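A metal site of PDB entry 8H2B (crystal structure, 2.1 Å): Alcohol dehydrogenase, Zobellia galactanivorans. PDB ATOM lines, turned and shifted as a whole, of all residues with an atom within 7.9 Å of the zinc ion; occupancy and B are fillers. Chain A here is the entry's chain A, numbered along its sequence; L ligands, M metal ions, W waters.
Thr 44 touches the zinc ion (OG1 to ZN, 3.8 Å). Of the 18 residues printed, 4 come within 4 Å of the zinc ion. Along chain A the residues within 4 Å of the zinc ion span positions 42 to 171.
The zinc ion is bound by a ring nitrogen (NE2) of His 59 (2.2 Å), the side-chain sulfur (SG) of Cys 171 (2.3 Å), the side-chain sulfur (SG) of Cys 42 (2.3 Å) and water W1 (2.5 Å).
A ring nitrogen (ND1) of His 59 lies within hydrogen-bond range of the side-chain carboxylate (OD1) of Asp 45 (2.8 Å). The side-chain sulfur (SG) of Cys 171 sits close to the indole nitrogen (NE1) of Trp 85, at 3.6 Å. The backbone carbonyl oxygen (O) of Cys 171 sits at hydrogen-bond distance from the side-chain hydroxyl (OG1) of Thr 175 (2.9 Å). The side-chain hydroxyl (OG1) of Thr 44 sits close to the side-chain sulfur (SG) of Cys 42 (3.6 Å). N of Cys 42 sits at hydrogen-bond distance from OD2 of Asp 45.
OG1 of Thr 44 lies within hydrogen-bond range of O13 of the ligand. N of His 43 sits at hydrogen-bond distance from O8 of the ligand, at 3.4 Å. N of Val 200 sits at hydrogen-bond distance from O9 of the ligand. N of Tyr 317 sits at hydrogen-bond distance from O14 of the ligand.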
ATOM      1  N   GLY A  40      -8.171 -20.366 -13.557  1.00  0.00           N
ATOM      2  CA  GLY A  40      -7.187 -20.457 -12.497  1.00  0.00           C
ATOM      3  C   GLY A  40      -7.149 -19.204 -11.631  1.00  0.00           C
ATOM      4  O   GLY A  40      -7.658 -18.141 -11.988  1.00  0.00           O
ATOM      5  N   LEU A  41      -6.550 -19.352 -10.448  1.00  0.00           N
ATOM      6  CA  LEU A  41      -6.351 -18.252  -9.517  1.00  0.00           C
ATOM      7  C   LEU A  41      -4.865 -17.974  -9.359  1.00  0.00           C
ATOM      8  O   LEU A  41      -4.072 -18.890  -9.123  1.00  0.00           O
ATOM      9  CB  LEU A  41      -6.981 -18.545  -8.168  1.00  0.00           C
ATOM     10  CG  LEU A  41      -8.433 -18.982  -8.320  1.00  0.00           C
ATOM     11  CD1 LEU A  41      -9.007 -19.385  -6.991  1.00  0.00           C
ATOM     12  CD2 LEU A  41      -9.239 -17.835  -8.948  1.00  0.00           C
ATOM     13  N   CYS A  42      -4.514 -16.703  -9.485  1.00  0.00           N
ATOM     14  CA  CYS A  42      -3.164 -16.192  -9.404  1.00  0.00           C
ATOM     15  C   CYS A  42      -3.089 -15.275  -8.198  1.00  0.00           C
ATOM     16  O   CYS A  42      -4.111 -14.729  -7.771  1.00  0.00           O
ATOM     17  CB  CYS A  42      -2.817 -15.452 -10.700  1.00  0.00           C
ATOM     18  SG  CYS A  42      -1.200 -14.734 -10.781  1.00  0.00           S
ATOM     19  N   HIS A  43      -1.892 -15.100  -7.620  1.00  0.00           N
ATOM     20  CA  HIS A  43      -1.763 -14.169  -6.509  1.00  0.00           C
ATOM     21  C   HIS A  43      -2.219 -12.768  -6.900  1.00  0.00           C
ATOM     22  O   HIS A  43      -2.744 -12.024  -6.059  1.00  0.00           O
ATOM     23  CB  HIS A  43      -0.313 -14.127  -5.994  1.00  0.00           C
ATOM     24  CG  HIS A  43      -0.155 -13.378  -4.690  1.00  0.00           C
ATOM     25  ND1 HIS A  43      -0.213 -12.007  -4.599  1.00  0.00           N
ATOM     26  CD2 HIS A  43       0.060 -13.828  -3.433  1.00  0.00           C
ATOM     27  CE1 HIS A  43      -0.047 -11.636  -3.352  1.00  0.00           C
ATOM     28  NE2 HIS A  43       0.122 -12.724  -2.609  1.00  0.00           N
ATOM     29  N   THR A  44      -2.064 -12.399  -8.186  1.00  0.00           N
ATOM     30  CA  THR A  44      -2.414 -11.062  -8.637  1.00  0.00           C
ATOM     31  C   THR A  44      -3.930 -10.807  -8.589  1.00  0.00           C
ATOM     32  O   THR A  44      -4.356  -9.660  -8.459  1.00  0.00           O
ATOM     33  CB  THR A  44      -1.872 -10.841 -10.049  1.00  0.00           C
ATOM     34  OG1 THR A  44      -0.506 -11.298 -10.104  1.00  0.00           O
ATOM     35  CG2 THR A  44      -1.924  -9.388 -10.448  1.00  0.00           C
ATOM     36  N   ASP A  45      -4.745 -11.867  -8.676  1.00  0.00           N
ATOM     37  CA  ASP A  45      -6.179 -11.669  -8.493  1.00  0.00           C
ATOM     38  C   ASP A  45      -6.471 -11.112  -7.108  1.00  0.00           C
ATOM     39  O   ASP A  45      -7.347 -10.246  -6.939  1.00  0.00           O
ATOM     40  CB  ASP A  45      -6.931 -12.978  -8.716  1.00  0.00           C
ATOM     41  CG  ASP A  45      -6.863 -13.437 -10.161  1.00  0.00           C
ATOM     42  OD1 ASP A  45      -7.042 -12.587 -11.064  1.00  0.00           O
ATOM     43  OD2 ASP A  45      -6.625 -14.637 -10.388  1.00  0.00           O
ATOM     44  N   ASP A  47      -4.312  -9.226  -5.366  1.00  0.00           N
ATOM     45  CA  ASP A  47      -3.935  -7.814  -5.443  1.00  0.00           C
ATOM     46  C   ASP A  47      -4.970  -6.998  -6.211  1.00  0.00           C
ATOM     47  O   ASP A  47      -5.072  -5.789  -5.987  1.00  0.00           O
ATOM     48  CB  ASP A  47      -2.556  -7.630  -6.099  1.00  0.00           C
ATOM     49  CG  ASP A  47      -1.492  -8.604  -5.584  1.00  0.00           C
ATOM     50  OD1 ASP A  47      -1.221  -8.605  -4.354  1.00  0.00           O
ATOM     51  OD2 ASP A  47      -0.935  -9.369  -6.399  1.00  0.00           O
ATOM     52  N   HIS A  59      -7.847 -13.814 -14.754  1.00  0.00           N
ATOM     53  CA  HIS A  59      -7.047 -13.649 -15.956  1.00  0.00           C
ATOM     54  C   HIS A  59      -6.328 -14.941 -16.295  1.00  0.00           C
ATOM     55  O   HIS A  59      -5.368 -14.928 -17.069  1.00  0.00           O
ATOM     56  CB  HIS A  59      -6.059 -12.505 -15.794  1.00  0.00           C
ATOM     57  CG  HIS A  59      -5.075 -12.726 -14.703  1.00  0.00           C
ATOM     58  ND1 HIS A  59      -5.411 -12.658 -13.373  1.00  0.00           N
ATOM     59  CD2 HIS A  59      -3.757 -13.046 -14.741  1.00  0.00           C
ATOM     60  CE1 HIS A  59      -4.346 -12.918 -12.634  1.00  0.00           C
ATOM     61  NE2 HIS A  59      -3.330 -13.152 -13.439  1.00  0.00           N
ATOM     62  N   GLU A  60      -6.760 -16.054 -15.728  1.00  0.00           N
ATOM     63  CA  GLU A  60      -6.356 -17.385 -16.141  1.00  0.00           C
ATOM     64  C   GLU A  60      -7.607 -18.133 -16.554  1.00  0.00           C
ATOM     65  O   GLU A  60      -8.600 -18.119 -15.818  1.00  0.00           O
ATOM     66  CB  GLU A  60      -5.636 -18.141 -15.022  1.00  0.00           C
ATOM     67  CG  GLU A  60      -4.219 -17.669 -14.707  1.00  0.00           C
ATOM     68  CD  GLU A  60      -3.548 -18.561 -13.655  1.00  0.00           C
ATOM     69  OE1 GLU A  60      -4.268 -19.343 -13.020  1.00  0.00           O
ATOM     70  OE2 GLU A  60      -2.303 -18.497 -13.476  1.00  0.00           O
ATOM     71  N   TRP A  85      -3.258 -12.908 -21.691  1.00  0.00           N
ATOM     72  CA  TRP A  85      -3.504 -11.495 -21.399  1.00  0.00           C
ATOM     73  C   TRP A  85      -2.490 -10.569 -22.056  1.00  0.00           C
ATOM     74  O   TRP A  85      -2.485  -9.383 -21.762  1.00  0.00           O
ATOM     75  CB  TRP A  85      -3.565 -11.224 -19.896  1.00  0.00           C
ATOM     76  CG  TRP A  85      -2.498 -11.770 -19.001  1.00  0.00           C
ATOM     77  CD1 TRP A  85      -2.545 -12.943 -18.281  1.00  0.00           C
ATOM     78  CD2 TRP A  85      -1.260 -11.129 -18.631  1.00  0.00           C
ATOM     79  NE1 TRP A  85      -1.401 -13.084 -17.525  1.00  0.00           N
ATOM     80  CE2 TRP A  85      -0.605 -11.976 -17.713  1.00  0.00           C
ATOM     81  CE3 TRP A  85      -0.645  -9.923 -18.994  1.00  0.00           C
ATOM     82  CZ2 TRP A  85       0.645 -11.664 -17.163  1.00  0.00           C
ATOM     83  CZ3 TRP A  85       0.597  -9.616 -18.445  1.00  0.00           C
ATOM     84  CH2 TRP A  85       1.221 -10.470 -17.535  1.00  0.00           C
ATOM     85  N   PHE A 137      -7.241  -7.746 -16.809  1.00  0.00           N
ATOM     86  CA  PHE A 137      -6.200  -8.137 -17.772  1.00  0.00           C
ATOM     87  C   PHE A 137      -6.771  -8.397 -19.169  1.00  0.00           C
ATOM     88  O   PHE A 137      -6.270  -9.251 -19.894  1.00  0.00           O
ATOM     89  CB  PHE A 137      -5.443  -9.379 -17.286  1.00  0.00           C
ATOM     90  CG  PHE A 137      -4.432  -9.102 -16.210  1.00  0.00           C
ATOM     91  CD1 PHE A 137      -4.841  -8.864 -14.901  1.00  0.00           C
ATOM     92  CD2 PHE A 137      -3.071  -9.085 -16.510  1.00  0.00           C
ATOM     93  CE1 PHE A 137      -3.911  -8.610 -13.897  1.00  0.00           C
ATOM     94  CE2 PHE A 137      -2.133  -8.841 -15.512  1.00  0.00           C
ATOM     95  CZ  PHE A 137      -2.558  -8.598 -14.199  1.00  0.00           C
ATOM     96  N   SER A 170      -2.484 -19.983 -18.717  1.00  0.00           N
ATOM     97  CA  SER A 170      -2.681 -18.556 -18.993  1.00  0.00           C
ATOM     98  C   SER A 170      -1.755 -17.636 -18.205  1.00  0.00           C
ATOM     99  O   SER A 170      -1.481 -16.525 -18.659  1.00  0.00           O
ATOM    100  CB  SER A 170      -4.121 -18.164 -18.676  1.00  0.00           C
ATOM    101  OG  SER A 170      -5.034 -18.807 -19.537  1.00  0.00           O
ATOM    102  N   CYS A 171      -1.363 -17.999 -16.991  1.00  0.00           N
ATOM    103  CA  CYS A 171      -0.485 -17.076 -16.283  1.00  0.00           C
ATOM    104  C   CYS A 171       0.646 -17.774 -15.525  1.00  0.00           C
ATOM    105  O   CYS A 171       1.823 -17.576 -15.849  1.00  0.00           O
ATOM    106  CB  CYS A 171      -1.258 -16.206 -15.312  1.00  0.00           C
ATOM    107  SG  CYS A 171      -0.237 -14.873 -14.660  1.00  0.00           S
ATOM    108  N   GLY A 172       0.303 -18.548 -14.498  1.00  0.00           N
ATOM    109  CA  GLY A 172       1.333 -19.123 -13.629  1.00  0.00           C
ATOM    110  C   GLY A 172       2.315 -19.990 -14.387  1.00  0.00           C
ATOM    111  O   GLY A 172       3.542 -19.849 -14.232  1.00  0.00           O
ATOM    112  N   THR A 175       4.285 -17.779 -17.092  1.00  0.00           N
ATOM    113  CA  THR A 175       5.224 -16.863 -16.450  1.00  0.00           C
ATOM    114  C   THR A 175       6.398 -17.628 -15.856  1.00  0.00           C
ATOM    115  O   THR A 175       7.555 -17.220 -16.022  1.00  0.00           O
ATOM    116  CB  THR A 175       4.520 -16.063 -15.355  1.00  0.00           C
ATOM    117  OG1 THR A 175       3.504 -15.216 -15.921  1.00  0.00           O
ATOM    118  CG2 THR A 175       5.533 -15.232 -14.574  1.00  0.00           C
ATOM    119  N   VAL A 200       3.688 -19.446  -9.256  1.00  0.00           N
ATOM    120  CA  VAL A 200       4.712 -19.218 -10.266  1.00  0.00           C
ATOM    121  C   VAL A 200       5.936 -20.083  -9.987  1.00  0.00           C
ATOM    122  O   VAL A 200       6.455 -20.759 -10.889  1.00  0.00           O
ATOM    123  CB  VAL A 200       5.073 -17.724 -10.325  1.00  0.00           C
ATOM    124  CG1 VAL A 200       6.285 -17.518 -11.187  1.00  0.00           C
ATOM    125  CG2 VAL A 200       3.884 -16.908 -10.861  1.00  0.00           C
ATOM    126  N   TYR A 317       5.463 -11.708 -17.763  1.00  0.00           N
ATOM    127  CA  TYR A 317       4.686 -12.785 -18.392  1.00  0.00           C
ATOM    128  C   TYR A 317       5.584 -13.799 -19.109  1.00  0.00           C
ATOM    129  O   TYR A 317       5.183 -14.439 -20.094  1.00  0.00           O
ATOM    130  CB  TYR A 317       3.639 -12.167 -19.309  1.00  0.00           C
ATOM    131  CG  TYR A 317       2.496 -13.018 -19.793  1.00  0.00           C
ATOM    132  CD1 TYR A 317       1.991 -14.047 -19.011  1.00  0.00           C
ATOM    133  CD2 TYR A 317       1.641 -12.525 -20.793  1.00  0.00           C
ATOM    134  CE1 TYR A 317       0.854 -14.741 -19.380  1.00  0.00           C
ATOM    135  CE2 TYR A 317       0.485 -13.190 -21.154  1.00  0.00           C
ATOM    136  CZ  TYR A 317       0.089 -14.285 -20.441  1.00  0.00           C
ATOM    137  OH  TYR A 317      -1.075 -14.943 -20.773  1.00  0.00           O
ATOM    138  N   LYS A 367      -1.956 -24.932  -7.268  1.00  0.00           N
ATOM    139  CA  LYS A 367      -2.926 -24.076  -7.930  1.00  0.00           C
ATOM    140  C   LYS A 367      -4.328 -24.558  -7.573  1.00  0.00           C
ATOM    141  O   LYS A 367      -4.593 -25.757  -7.589  1.00  0.00           O
ATOM    142  CB  LYS A 367      -2.743 -24.089  -9.459  1.00  0.00           C
ATOM    143  CG  LYS A 367      -1.705 -23.128 -10.031  1.00  0.00           C
ATOM    144  CD  LYS A 367      -2.131 -21.681  -9.898  1.00  0.00           C
ATOM    145  CE  LYS A 367      -1.342 -20.773 -10.844  1.00  0.00           C
ATOM    146  NZ  LYS A 367      -1.869 -19.381 -10.836  1.00  0.00           N
HETATM  147  P1  LIG L   1       1.949 -17.381  -4.308  1.00  0.00           P
HETATM  148  O1  LIG L   1       1.302 -16.743  -3.124  1.00  0.00           O
HETATM  149  O2  LIG L   1       1.240 -18.600  -4.839  1.00  0.00           O
HETATM  150  O3  LIG L   1       3.510 -17.857  -3.977  1.00  0.00           O
HETATM  151  C1  LIG L   1       4.294 -17.024  -3.159  1.00  0.00           C
HETATM  152  C2  LIG L   1       5.298 -18.039  -2.491  1.00  0.00           C
HETATM  153  O4  LIG L   1       6.304 -17.359  -1.986  1.00  0.00           O
HETATM  154  C3  LIG L   1       4.597 -18.774  -1.346  1.00  0.00           C
HETATM  155  O5  LIG L   1       4.811 -20.129  -1.361  1.00  0.00           O
HETATM  156  C4  LIG L   1       5.276 -18.159  -0.098  1.00  0.00           C
HETATM  157  O6  LIG L   1       5.186 -19.177   0.978  1.00  0.00           O
HETATM  158  C5  LIG L   1       6.491 -17.962  -0.507  1.00  0.00           C
HETATM  159  N1  LIG L   1       7.272 -17.028   0.329  1.00  0.00           N
HETATM  160  C6  LIG L   1       6.724 -15.988   0.952  1.00  0.00           C
HETATM  161  N2  LIG L   1       7.701 -15.352   1.652  1.00  0.00           N
HETATM  162  C7  LIG L   1       8.846 -16.030   1.454  1.00  0.00           C
HETATM  163  C8  LIG L   1      10.137 -15.825   1.925  1.00  0.00           C
HETATM  164  N3  LIG L   1      10.582 -14.755   2.819  1.00  0.00           N
HETATM  165  N4  LIG L   1      11.111 -16.646   1.560  1.00  0.00           N
HETATM  166  C9  LIG L   1      10.843 -17.695   0.725  1.00  0.00           C
HETATM  167  N5  LIG L   1       9.578 -17.907   0.264  1.00  0.00           N
HETATM  168  C10 LIG L   1       8.588 -17.058   0.628  1.00  0.00           C
HETATM  169  O7  LIG L   1       1.974 -16.250  -5.464  1.00  0.00           O
HETATM  170  P2  LIG L   1       2.297 -16.530  -7.035  1.00  0.00           P
HETATM  171  O8  LIG L   1       1.001 -16.821  -7.744  1.00  0.00           O
HETATM  172  O9  LIG L   1       3.261 -17.686  -7.204  1.00  0.00           O
HETATM  173  O10 LIG L   1       2.954 -15.135  -7.549  1.00  0.00           O
HETATM  174  C11 LIG L   1       4.142 -14.677  -7.000  1.00  0.00           C
HETATM  175  C12 LIG L   1       4.427 -13.320  -7.542  1.00  0.00           C
HETATM  176  O11 LIG L   1       4.602 -13.321  -8.851  1.00  0.00           O
HETATM  177  C13 LIG L   1       3.148 -12.323  -7.237  1.00  0.00           C
HETATM  178  O12 LIG L   1       3.741 -11.094  -6.679  1.00  0.00           O
HETATM  179  C14 LIG L   1       2.569 -12.132  -8.338  1.00  0.00           C
HETATM  180  O13 LIG L   1       1.954 -10.768  -8.404  1.00  0.00           O
HETATM  181  C15 LIG L   1       3.759 -12.212  -9.406  1.00  0.00           C
HETATM  182  N6  LIG L   1       3.446 -12.526 -10.680  1.00  0.00           N
HETATM  183  C16 LIG L   1       4.178 -11.927 -11.665  1.00  0.00           C
HETATM  184  C17 LIG L   1       3.954 -12.257 -13.004  1.00  0.00           C
HETATM  185  C18 LIG L   1       4.814 -11.548 -14.095  1.00  0.00           C
HETATM  186  O14 LIG L   1       4.399 -11.472 -15.215  1.00  0.00           O
HETATM  187  N7  LIG L   1       6.145 -10.994 -13.761  1.00  0.00           N
HETATM  188  C19 LIG L   1       2.997 -13.171 -13.320  1.00  0.00           C
HETATM  189  C20 LIG L   1       2.273 -13.781 -12.341  1.00  0.00           C
HETATM  190  C21 LIG L   1       2.504 -13.446 -11.000  1.00  0.00           C
HETATM  191 ZN    ZN M   1      -1.234 -13.757 -12.904  1.00  0.00          ZN
HETATM  192  O   HOH W   1      -0.129 -11.556 -13.037  1.00  0.00           O
